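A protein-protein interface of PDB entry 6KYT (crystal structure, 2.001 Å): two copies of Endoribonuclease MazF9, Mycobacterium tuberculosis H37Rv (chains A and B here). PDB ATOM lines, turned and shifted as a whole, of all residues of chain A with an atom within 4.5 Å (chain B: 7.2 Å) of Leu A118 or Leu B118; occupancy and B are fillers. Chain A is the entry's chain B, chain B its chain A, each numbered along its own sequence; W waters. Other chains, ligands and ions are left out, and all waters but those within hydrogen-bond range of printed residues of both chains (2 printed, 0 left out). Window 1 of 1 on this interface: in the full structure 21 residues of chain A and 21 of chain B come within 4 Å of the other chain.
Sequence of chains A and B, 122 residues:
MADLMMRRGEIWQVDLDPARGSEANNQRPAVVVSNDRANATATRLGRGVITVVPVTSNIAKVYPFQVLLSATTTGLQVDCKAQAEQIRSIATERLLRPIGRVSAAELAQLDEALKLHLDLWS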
ATOM      1  N   ARG A   8     -10.354   6.763  34.074  1.00  0.00           N
ATOM      2  CA  ARG A   8     -10.645   6.032  32.847  1.00  0.00           C
ATOM      3  C   ARG A   8     -11.640   4.908  33.106  1.00  0.00           C
ATOM      4  O   ARG A   8     -11.562   4.205  34.117  1.00  0.00           O
ATOM      5  CB  ARG A   8      -9.357   5.469  32.246  1.00  0.00           C
ATOM      6  CG  ARG A   8      -9.493   5.073  30.788  1.00  0.00           C
ATOM      7  CD  ARG A   8      -8.172   4.607  30.203  1.00  0.00           C
ATOM      8  NE  ARG A   8      -8.250   4.475  28.750  1.00  0.00           N
ATOM      9  CZ  ARG A   8      -8.631   3.369  28.122  1.00  0.00           C
ATOM     10  NH1 ARG A   8      -8.975   2.295  28.818  1.00  0.00           N
ATOM     11  NH2 ARG A   8      -8.673   3.338  26.796  1.00  0.00           N
ATOM     12  N   VAL A  33     -11.605   8.093  28.502  1.00  0.00           N
ATOM     13  CA  VAL A  33     -10.650   7.174  27.888  1.00  0.00           C
ATOM     14  C   VAL A  33      -9.238   7.746  27.913  1.00  0.00           C
ATOM     15  O   VAL A  33      -8.280   7.067  27.528  1.00  0.00           O
ATOM     16  CB  VAL A  33     -11.060   6.813  26.448  1.00  0.00           C
ATOM     17  CG1 VAL A  33     -12.356   6.018  26.447  1.00  0.00           C
ATOM     18  CG2 VAL A  33     -11.194   8.066  25.600  1.00  0.00           C
ATOM     19  N   THR A  51     -10.327  13.206  27.558  1.00  0.00           N
ATOM     20  CA  THR A  51     -10.796  12.652  26.296  1.00  0.00           C
ATOM     21  C   THR A  51     -11.865  11.617  26.597  1.00  0.00           C
ATOM     22  O   THR A  51     -11.668  10.747  27.451  1.00  0.00           O
ATOM     23  CB  THR A  51      -9.654  12.029  25.487  1.00  0.00           C
ATOM     24  OG1 THR A  51      -8.580  12.970  25.370  1.00  0.00           O
ATOM     25  CG2 THR A  51     -10.135  11.663  24.094  1.00  0.00           C
ATOM     26  N   ILE A  87     -14.989   9.917  19.459  1.00  0.00           N
ATOM     27  CA  ILE A  87     -14.071  10.296  20.526  1.00  0.00           C
ATOM     28  C   ILE A  87     -13.682  11.763  20.395  1.00  0.00           C
ATOM     29  O   ILE A  87     -13.510  12.284  19.287  1.00  0.00           O
ATOM     30  CB  ILE A  87     -12.835   9.378  20.497  1.00  0.00           C
ATOM     31  CG1 ILE A  87     -11.841   9.761  21.596  1.00  0.00           C
ATOM     32  CG2 ILE A  87     -12.162   9.417  19.129  1.00  0.00           C
ATOM     33  CD1 ILE A  87     -10.594   8.902  21.619  1.00  0.00           C
ATOM     34  N   LEU A 114     -11.491   1.362  20.059  1.00  0.00           N
ATOM     35  CA  LEU A 114     -10.618   2.511  19.841  1.00  0.00           C
ATOM     36  C   LEU A 114      -9.442   2.145  18.943  1.00  0.00           C
ATOM     37  O   LEU A 114      -9.109   2.890  18.013  1.00  0.00           O
ATOM     38  CB  LEU A 114     -10.126   3.053  21.180  1.00  0.00           C
ATOM     39  CG  LEU A 114     -11.147   3.836  22.009  1.00  0.00           C
ATOM     40  CD1 LEU A 114     -10.656   4.010  23.437  1.00  0.00           C
ATOM     41  CD2 LEU A 114     -11.425   5.187  21.367  1.00  0.00           C
ATOM     42  N   LYS A 115      -8.804   0.999  19.206  1.00  0.00           N
ATOM     43  CA  LYS A 115      -7.691   0.566  18.366  1.00  0.00           C
ATOM     44  C   LYS A 115      -8.127   0.395  16.916  1.00  0.00           C
ATOM     45  O   LYS A 115      -7.381   0.737  15.991  1.00  0.00           O
ATOM     46  CB  LYS A 115      -7.100  -0.734  18.914  1.00  0.00           C
ATOM     47  CG  LYS A 115      -6.182  -0.531  20.114  1.00  0.00           C
ATOM     48  CD  LYS A 115      -6.122  -1.769  20.999  1.00  0.00           C
ATOM     49  CE  LYS A 115      -5.392  -2.917  20.326  1.00  0.00           C
ATOM     50  NZ  LYS A 115      -3.913  -2.768  20.413  1.00  0.00           N
ATOM     51  N   LEU A 116      -9.341  -0.116  16.697  1.00  0.00           N
ATOM     52  CA  LEU A 116      -9.842  -0.275  15.335  1.00  0.00           C
ATOM     53  C   LEU A 116     -10.102   1.076  14.683  1.00  0.00           C
ATOM     54  O   LEU A 116      -9.665   1.325  13.553  1.00  0.00           O
ATOM     55  CB  LEU A 116     -11.115  -1.122  15.334  1.00  0.00           C
ATOM     56  CG  LEU A 116     -11.765  -1.314  13.960  1.00  0.00           C
ATOM     57  CD1 LEU A 116     -10.946  -2.267  13.103  1.00  0.00           C
ATOM     58  CD2 LEU A 116     -13.201  -1.801  14.092  1.00  0.00           C
ATOM     59  N   HIS A 117     -10.818   1.963  15.380  1.00  0.00           N
ATOM     60  CA  HIS A 117     -11.180   3.248  14.789  1.00  0.00           C
ATOM     61  C   HIS A 117      -9.947   4.081  14.465  1.00  0.00           C
ATOM     62  O   HIS A 117      -9.910   4.775  13.442  1.00  0.00           O
ATOM     63  CB  HIS A 117     -12.110   4.021  15.724  1.00  0.00           C
ATOM     64  CG  HIS A 117     -12.401   5.415  15.260  1.00  0.00           C
ATOM     65  ND1 HIS A 117     -13.136   5.683  14.126  1.00  0.00           N
ATOM     66  CD2 HIS A 117     -12.046   6.617  15.771  1.00  0.00           C
ATOM     67  CE1 HIS A 117     -13.226   6.991  13.961  1.00  0.00           C
ATOM     68  NE2 HIS A 117     -12.574   7.580  14.946  1.00  0.00           N
ATOM     69  N   LEU A 118      -8.926   4.028  15.319  1.00  0.00           N
ATOM     70  CA  LEU A 118      -7.738   4.849  15.146  1.00  0.00           C
ATOM     71  C   LEU A 118      -6.595   4.107  14.466  1.00  0.00           C
ATOM     72  O   LEU A 118      -5.470   4.619  14.437  1.00  0.00           O
ATOM     73  CB  LEU A 118      -7.282   5.398  16.497  1.00  0.00           C
ATOM     74  CG  LEU A 118      -8.290   6.356  17.134  1.00  0.00           C
ATOM     75  CD1 LEU A 118      -7.891   6.673  18.558  1.00  0.00           C
ATOM     76  CD2 LEU A 118      -8.407   7.628  16.308  1.00  0.00           C
ATOM     77  N   ASP A 119      -6.860   2.920  13.914  1.00  0.00           N
ATOM     78  CA  ASP A 119      -5.860   2.144  13.179  1.00  0.00           C
ATOM     79  C   ASP A 119      -4.631   1.868  14.042  1.00  0.00           C
ATOM     80  O   ASP A 119      -3.490   1.981  13.589  1.00  0.00           O
ATOM     81  CB  ASP A 119      -5.466   2.845  11.876  1.00  0.00           C
ATOM     82  CG  ASP A 119      -5.002   1.875  10.808  1.00  0.00           C
ATOM     83  OD1 ASP A 119      -4.801   0.685  11.130  1.00  0.00           O
ATOM     84  OD2 ASP A 119      -4.834   2.304   9.648  1.00  0.00           O
ATOM     85  N   LEU A 120      -4.868   1.507  15.303  1.00  0.00           N
ATOM     86  CA  LEU A 120      -3.798   1.210  16.245  1.00  0.00           C
ATOM     87  C   LEU A 120      -3.670  -0.280  16.538  1.00  0.00           C
ATOM     88  O   LEU A 120      -2.905  -0.660  17.431  1.00  0.00           O
ATOM     89  CB  LEU A 120      -4.002   1.988  17.547  1.00  0.00           C
ATOM     90  CG  LEU A 120      -4.084   3.511  17.418  1.00  0.00           C
ATOM     91  CD1 LEU A 120      -4.450   4.145  18.751  1.00  0.00           C
ATOM     92  CD2 LEU A 120      -2.776   4.084  16.891  1.00  0.00           C
ATOM     93  N   ARG B   8      -5.441   8.657   6.437  1.00  0.00           N
ATOM     94  CA  ARG B   8      -4.753   8.814   7.709  1.00  0.00           C
ATOM     95  C   ARG B   8      -3.341   9.338   7.491  1.00  0.00           C
ATOM     96  O   ARG B   8      -2.608   8.849   6.626  1.00  0.00           O
ATOM     97  CB  ARG B   8      -4.717   7.473   8.442  1.00  0.00           C
ATOM     98  CG  ARG B   8      -4.391   7.573   9.915  1.00  0.00           C
ATOM     99  CD  ARG B   8      -4.699   6.269  10.626  1.00  0.00           C
ATOM    100  NE  ARG B   8      -4.463   6.365  12.061  1.00  0.00           N
ATOM    101  CZ  ARG B   8      -3.280   6.173  12.634  1.00  0.00           C
ATOM    102  NH1 ARG B   8      -2.224   5.875  11.890  1.00  0.00           N
ATOM    103  NH2 ARG B   8      -3.153   6.281  13.949  1.00  0.00           N
ATOM    104  N   VAL B  33      -6.484  11.015  11.770  1.00  0.00           N
ATOM    105  CA  VAL B  33      -6.071   9.813  12.489  1.00  0.00           C
ATOM    106  C   VAL B  33      -7.122   8.711  12.475  1.00  0.00           C
ATOM    107  O   VAL B  33      -6.790   7.565  12.816  1.00  0.00           O
ATOM    108  CB  VAL B  33      -5.662  10.130  13.944  1.00  0.00           C
ATOM    109  CG1 VAL B  33      -4.400  10.981  13.965  1.00  0.00           C
ATOM    110  CG2 VAL B  33      -6.795  10.826  14.683  1.00  0.00           C
ATOM    111  N   SER B  34      -8.367   9.002  12.110  1.00  0.00           N
ATOM    112  CA  SER B  34      -9.335   7.934  11.905  1.00  0.00           C
ATOM    113  C   SER B  34      -8.940   7.115  10.681  1.00  0.00           C
ATOM    114  O   SER B  34      -8.350   7.633   9.729  1.00  0.00           O
ATOM    115  CB  SER B  34     -10.744   8.504  11.733  1.00  0.00           C
ATOM    116  OG  SER B  34     -10.745   9.604  10.842  1.00  0.00           O
ATOM    117  N   ASN B  35      -9.259   5.823  10.713  1.00  0.00           N
ATOM    118  CA  ASN B  35      -8.767   4.939   9.669  1.00  0.00           C
ATOM    119  C   ASN B  35      -9.415   5.273   8.325  1.00  0.00           C
ATOM    120  O   ASN B  35     -10.487   5.886   8.245  1.00  0.00           O
ATOM    121  CB  ASN B  35      -8.989   3.468  10.041  1.00  0.00           C
ATOM    122  CG  ASN B  35     -10.449   3.052  10.002  1.00  0.00           C
ATOM    123  OD1 ASN B  35     -11.059   2.963   8.936  1.00  0.00           O
ATOM    124  ND2 ASN B  35     -11.010   2.768  11.171  1.00  0.00           N
ATOM    125  N   THR B  51     -11.907  11.973  12.637  1.00  0.00           N
ATOM    126  CA  THR B  51     -11.131  12.174  13.854  1.00  0.00           C
ATOM    127  C   THR B  51      -9.760  12.734  13.490  1.00  0.00           C
ATOM    128  O   THR B  51      -9.012  12.117  12.723  1.00  0.00           O
ATOM    129  CB  THR B  51     -10.996  10.871  14.637  1.00  0.00           C
ATOM    130  OG1 THR B  51     -12.298  10.326  14.883  1.00  0.00           O
ATOM    131  CG2 THR B  51     -10.312  11.126  15.968  1.00  0.00           C
ATOM    132  N   VAL B  52      -9.437  13.906  14.040  1.00  0.00           N
ATOM    133  CA  VAL B  52      -8.209  14.622  13.730  1.00  0.00           C
ATOM    134  C   VAL B  52      -7.489  14.991  15.020  1.00  0.00           C
ATOM    135  O   VAL B  52      -8.065  14.999  16.112  1.00  0.00           O
ATOM    136  CB  VAL B  52      -8.471  15.893  12.891  1.00  0.00           C
ATOM    137  CG1 VAL B  52      -9.276  15.561  11.642  1.00  0.00           C
ATOM    138  CG2 VAL B  52      -9.179  16.946  13.732  1.00  0.00           C
ATOM    139  N   VAL B  53      -6.208  15.304  14.868  1.00  0.00           N
ATOM    140  CA  VAL B  53      -5.341  15.769  15.941  1.00  0.00           C
ATOM    141  C   VAL B  53      -4.902  17.186  15.589  1.00  0.00           C
ATOM    142  O   VAL B  53      -4.323  17.404  14.519  1.00  0.00           O
ATOM    143  CB  VAL B  53      -4.121  14.853  16.135  1.00  0.00           C
ATOM    144  CG1 VAL B  53      -3.107  15.511  17.049  1.00  0.00           C
ATOM    145  CG2 VAL B  53      -4.555  13.505  16.690  1.00  0.00           C
ATOM    146  N   ALA B  84      -1.673  15.164  20.293  1.00  0.00           N
ATOM    147  CA  ALA B  84      -2.562  14.012  20.409  1.00  0.00           C
ATOM    148  C   ALA B  84      -3.453  14.091  21.641  1.00  0.00           C
ATOM    149  O   ALA B  84      -4.521  13.469  21.659  1.00  0.00           O
ATOM    150  CB  ALA B  84      -1.754  12.714  20.431  1.00  0.00           C
ATOM    151  N   ILE B  87      -7.087  15.351  20.696  1.00  0.00           N
ATOM    152  CA  ILE B  87      -7.778  14.654  19.618  1.00  0.00           C
ATOM    153  C   ILE B  87      -9.263  15.000  19.632  1.00  0.00           C
ATOM    154  O   ILE B  87      -9.880  15.130  20.694  1.00  0.00           O
ATOM    155  CB  ILE B  87      -7.538  13.138  19.755  1.00  0.00           C
ATOM    156  CG1 ILE B  87      -8.223  12.361  18.631  1.00  0.00           C
ATOM    157  CG2 ILE B  87      -7.995  12.639  21.123  1.00  0.00           C
ATOM    158  CD1 ILE B  87      -7.964  10.868  18.696  1.00  0.00           C
ATOM    159  N   SER B  89     -13.061  14.506  17.143  1.00  0.00           N
ATOM    160  CA  SER B  89     -13.835  14.088  15.981  1.00  0.00           C
ATOM    161  C   SER B  89     -14.763  15.226  15.570  1.00  0.00           C
ATOM    162  O   SER B  89     -15.550  15.718  16.386  1.00  0.00           O
ATOM    163  CB  SER B  89     -14.636  12.820  16.277  1.00  0.00           C
ATOM    164  OG  SER B  89     -13.773  11.721  16.516  1.00  0.00           O
ATOM    165  N   ASP B 111       1.080   7.256  16.234  1.00  0.00           N
ATOM    166  CA  ASP B 111       0.464   6.048  16.772  1.00  0.00           C
ATOM    167  C   ASP B 111       0.867   5.838  18.226  1.00  0.00           C
ATOM    168  O   ASP B 111       0.016   5.595  19.092  1.00  0.00           O
ATOM    169  CB  ASP B 111       0.854   4.832  15.928  1.00  0.00           C
ATOM    170  CG  ASP B 111       0.333   4.913  14.507  1.00  0.00           C
ATOM    171  OD1 ASP B 111      -0.538   5.765  14.236  1.00  0.00           O
ATOM    172  OD2 ASP B 111       0.795   4.116  13.661  1.00  0.00           O
ATOM    173  N   GLU B 112       2.169   5.945  18.514  1.00  0.00           N
ATOM    174  CA  GLU B 112       2.633   5.759  19.885  1.00  0.00           C
ATOM    175  C   GLU B 112       2.058   6.820  20.820  1.00  0.00           C
ATOM    176  O   GLU B 112       1.672   6.513  21.955  1.00  0.00           O
ATOM    177  CB  GLU B 112       4.160   5.774  19.930  1.00  0.00           C
ATOM    178  CG  GLU B 112       4.799   4.573  19.255  1.00  0.00           C
ATOM    179  CD  GLU B 112       4.199   3.261  19.724  1.00  0.00           C
ATOM    180  OE1 GLU B 112       3.599   2.547  18.892  1.00  0.00           O
ATOM    181  OE2 GLU B 112       4.322   2.947  20.925  1.00  0.00           O
ATOM    182  N   ALA B 113       1.992   8.073  20.361  1.00  0.00           N
ATOM    183  CA  ALA B 113       1.442   9.136  21.198  1.00  0.00           C
ATOM    184  C   ALA B 113      -0.037   8.902  21.485  1.00  0.00           C
ATOM    185  O   ALA B 113      -0.514   9.177  22.594  1.00  0.00           O
ATOM    186  CB  ALA B 113       1.653  10.494  20.530  1.00  0.00           C
ATOM    187  N   LEU B 114      -0.777   8.390  20.498  1.00  0.00           N
ATOM    188  CA  LEU B 114      -2.192   8.106  20.707  1.00  0.00           C
ATOM    189  C   LEU B 114      -2.388   6.953  21.685  1.00  0.00           C
ATOM    190  O   LEU B 114      -3.250   7.025  22.570  1.00  0.00           O
ATOM    191  CB  LEU B 114      -2.867   7.804  19.370  1.00  0.00           C
ATOM    192  CG  LEU B 114      -3.071   9.003  18.441  1.00  0.00           C
ATOM    193  CD1 LEU B 114      -3.414   8.543  17.030  1.00  0.00           C
ATOM    194  CD2 LEU B 114      -4.153   9.922  18.988  1.00  0.00           C
ATOM    195  N   LYS B 115      -1.597   5.883  21.543  1.00  0.00           N
ATOM    196  CA  LYS B 115      -1.672   4.789  22.509  1.00  0.00           C
ATOM    197  C   LYS B 115      -1.320   5.268  23.911  1.00  0.00           C
ATOM    198  O   LYS B 115      -1.914   4.814  24.898  1.00  0.00           O
ATOM    199  CB  LYS B 115      -0.743   3.648  22.101  1.00  0.00           C
ATOM    200  CG  LYS B 115      -1.070   2.993  20.777  1.00  0.00           C
ATOM    201  CD  LYS B 115      -0.022   1.942  20.463  1.00  0.00           C
ATOM    202  CE  LYS B 115      -0.130   1.443  19.038  1.00  0.00           C
ATOM    203  NZ  LYS B 115       1.009   0.542  18.711  1.00  0.00           N
ATOM    204  N   LEU B 116      -0.348   6.176  24.020  1.00  0.00           N
ATOM    205  CA  LEU B 116       0.031   6.704  25.327  1.00  0.00           C
ATOM    206  C   LEU B 116      -1.106   7.510  25.941  1.00  0.00           C
ATOM    207  O   LEU B 116      -1.489   7.287  27.096  1.00  0.00           O
ATOM    208  CB  LEU B 116       1.288   7.564  25.204  1.00  0.00           C
ATOM    209  CG  LEU B 116       1.660   8.351  26.464  1.00  0.00           C
ATOM    210  CD1 LEU B 116       2.085   7.420  27.593  1.00  0.00           C
ATOM    211  CD2 LEU B 116       2.744   9.374  26.166  1.00  0.00           C
ATOM    212  N   HIS B 117      -1.661   8.457  25.179  1.00  0.00           N
ATOM    213  CA  HIS B 117      -2.696   9.329  25.723  1.00  0.00           C
ATOM    214  C   HIS B 117      -3.962   8.552  26.061  1.00  0.00           C
ATOM    215  O   HIS B 117      -4.631   8.847  27.057  1.00  0.00           O
ATOM    216  CB  HIS B 117      -3.015  10.453  24.737  1.00  0.00           C
ATOM    217  CG  HIS B 117      -4.090  11.381  25.211  1.00  0.00           C
ATOM    218  ND1 HIS B 117      -3.925  12.217  26.294  1.00  0.00           N
ATOM    219  CD2 HIS B 117      -5.348  11.593  24.759  1.00  0.00           C
ATOM    220  CE1 HIS B 117      -5.033  12.913  26.483  1.00  0.00           C
ATOM    221  NE2 HIS B 117      -5.913  12.552  25.566  1.00  0.00           N
ATOM    222  N   LEU B 118      -4.307   7.556  25.246  1.00  0.00           N
ATOM    223  CA  LEU B 118      -5.551   6.819  25.421  1.00  0.00           C
ATOM    224  C   LEU B 118      -5.376   5.517  26.193  1.00  0.00           C
ATOM    225  O   LEU B 118      -6.351   4.773  26.346  1.00  0.00           O
ATOM    226  CB  LEU B 118      -6.186   6.537  24.058  1.00  0.00           C
ATOM    227  CG  LEU B 118      -6.523   7.802  23.268  1.00  0.00           C
ATOM    228  CD1 LEU B 118      -7.104   7.447  21.917  1.00  0.00           C
ATOM    229  CD2 LEU B 118      -7.483   8.683  24.054  1.00  0.00           C
ATOM    230  N   ASP B 119      -4.167   5.229  26.680  1.00  0.00           N
ATOM    231  CA  ASP B 119      -3.903   4.062  27.527  1.00  0.00           C
ATOM    232  C   ASP B 119      -4.246   2.762  26.799  1.00  0.00           C
ATOM    233  O   ASP B 119      -4.896   1.869  27.345  1.00  0.00           O
ATOM    234  CB  ASP B 119      -4.661   4.170  28.853  1.00  0.00           C
ATOM    235  CG  ASP B 119      -3.834   3.713  30.038  1.00  0.00           C
ATOM    236  OD1 ASP B 119      -2.591   3.692  29.922  1.00  0.00           O
ATOM    237  OD2 ASP B 119      -4.425   3.384  31.088  1.00  0.00           O
ATOM    238  N   LEU B 120      -3.794   2.658  25.553  1.00  0.00           N
ATOM    239  CA  LEU B 120      -4.118   1.528  24.690  1.00  0.00           C
ATOM    240  C   LEU B 120      -2.908   0.611  24.567  1.00  0.00           C
ATOM    241  O   LEU B 120      -1.823   1.055  24.177  1.00  0.00           O
ATOM    242  CB  LEU B 120      -4.569   2.013  23.314  1.00  0.00           C
ATOM    243  CG  LEU B 120      -5.849   2.851  23.318  1.00  0.00           C
ATOM    244  CD1 LEU B 120      -6.168   3.369  21.926  1.00  0.00           C
ATOM    245  CD2 LEU B 120      -7.014   2.045  23.872  1.00  0.00           C
ATOM    246  N   TRP B 121      -3.101  -0.665  24.892  1.00  0.00           N
ATOM    247  CA  TRP B 121      -2.037  -1.650  24.778  1.00  0.00           C
ATOM    248  C   TRP B 121      -1.800  -2.019  23.315  1.00  0.00           C
ATOM    249  O   TRP B 121      -2.662  -1.839  22.449  1.00  0.00           O
ATOM    250  CB  TRP B 121      -2.384  -2.904  25.581  1.00  0.00           C
ATOM    251  CG  TRP B 121      -3.617  -3.600  25.087  1.00  0.00           C
ATOM    252  CD1 TRP B 121      -4.901  -3.384  25.496  1.00  0.00           C
ATOM    253  CD2 TRP B 121      -3.683  -4.623  24.084  1.00  0.00           C
ATOM    254  NE1 TRP B 121      -5.761  -4.209  24.813  1.00  0.00           N
ATOM    255  CE2 TRP B 121      -5.039  -4.980  23.940  1.00  0.00           C
ATOM    256  CE3 TRP B 121      -2.727  -5.272  23.296  1.00  0.00           C
ATOM    257  CZ2 TRP B 121      -5.462  -5.956  23.039  1.00  0.00           C
ATOM    258  CZ3 TRP B 121      -3.150  -6.242  22.403  1.00  0.00           C
ATOM    259  CH2 TRP B 121      -4.505  -6.574  22.282  1.00  0.00           C
HETATM  260  O   HOH W   1      -1.208   2.415  12.579  1.00  0.00           O
HETATM  261  O   HOH W   2      -1.954   4.107   9.391  1.00  0.00           O
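NE of Arg B8 sits at hydrogen-bond distance from O of Val B33, at 2.7 Å. N of Val B33 sits at hydrogen-bond distance from O of Thr B51, 2.9 Å away. OG of Ser B34 lies within hydrogen-bond range of N of Thr B51 (3.2 Å). The side-chain hydroxyl (OG) of Ser B89 is in hydrogen-bond range of the side-chain hydroxyl (OG1) of Thr B51. The side-chain amino group (NZ) of Lys B115 is in salt-bridge range of the side-chain carboxylate (OE1) of Glu B112, at 3.3 Å. The backbone carbonyl oxygen of Lys A115 lies within hydrogen-bond range of the backbone NH of Leu A120, at 2.7 Å.
Thr A51 touches Ile B87. CD2 of Leu B118 touches CG2 of Thr A51, 3.99 Å away. CD1 of Leu B118 touches CD1 of Ile A87, 3.8 Å away. His A117 touches Ser B34. CG2 of Thr B51 touches CD2 of Leu A118 (3.998 Å). Leu A118 touches Leu B118. Leu A120 touches Arg B8. Asp B111 touches Leu A120 (CA to CD2, 3.8 Å). Leu A120 touches Lys B115. CD1 of Leu A120 touches CD1 of Leu B120, 3.7 Å away.
Of the printed residues of chain B, Ile A87 touches Ser B89 (2.8 Å) and Leu B118 (3.8 Å). Of the printed residues of chain B, His A117 touches Ser B34 (3.6 Å), Asn B35 (3.0 Å) and Thr B51 (2.8 Å). Printed residues of chain B within 4 Å of Leu A118: Arg B8, Val B33, Thr B51 and Leu B118. Of the printed residues of chain B, Asp A119 touches Arg B8 (3.7 Å). Of the printed residues of chain B, Leu A120 touches Arg B8 (3.7 Å), Asp B111 (3.8 Å), Lys B115 (3.8 Å) and Leu B120 (3.7 Å). Of the printed residues of chain A, Ser B34 touches His A117. Of the printed residues of chain A, Leu B118 touches Arg A8, Val A33, Thr A51, Ile A87 and Leu A118. The nearest printed residue of chain A that does not touch Leu B118 is Leu A114 (4.9 Å). The nearest printed residue of chain A that does not touch Val B33 is His A117 (4.2 Å).
Of the 21 printed residues of chain B, 14 touch a printed residue of chain A. Hydrophobic or aromatic side chains of chain B within 4 Å of the printed part of chain A: Val B33, Ile B87, His B117, Leu B118, Leu B120 and Trp B121. Hydrophobic or aromatic side chains of chain A within 4 Å of the printed part of chain B: Ile A87, His A117, Leu A118 and Leu A120.
Water W1 lies within hydrogen-bond range of O of Asp A119 (2.5 Å) and OD2 of Asp B111 (2.8 Å). Water W2 bridges the guanidinium group (NH1) of Arg B8 (3.1 Å) and the side-chain carboxylate (OD2) of Asp A119 (3.4 Å).
Arg A8 touches Leu B120, and with the chains exchanged Leu A120 touches Arg B8. Thr A51 touches His B117, and with the chains exchanged His A117 touches Thr B51. Thr A51 touches Leu B118, and with the chains exchanged Leu A118 touches Thr B51. Ile A87 touches Leu B118, but with the chains exchanged Leu A118 does not touch Ile B87 (4.05 Å).
NH2 of Arg B8 lies within hydrogen-bond range of O of Leu A118. ND2 of Asn B35 sits at hydrogen-bond distance from O of Leu A116. The backbone carbonyl oxygen (O) of His A117 sits at hydrogen-bond distance from the backbone NH (N) of Asn B35 (3.0 Å). NE2 of His A117 is in hydrogen-bond range of OG1 of Thr B51 (2.8 Å). The side-chain hydroxyl (OG) of Ser B89 sits at hydrogen-bond distance from the backbone carbonyl oxygen (O) of Ile A87 (2.8 Å). A ring nitrogen (NE2) of His B117 lies within hydrogen-bond range of the side-chain hydroxyl (OG1) of Thr A51, 2.7 Å away. O of Leu B118 sits at hydrogen-bond distance from NH2 of Arg A8 (2.8 Å). The side-chain amino group of Lys A115 lies within hydrogen-bond range of the backbone carbonyl oxygen of Trp B121. O of Val A33 lies close to O of Leu B118, 3.2 Å away.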
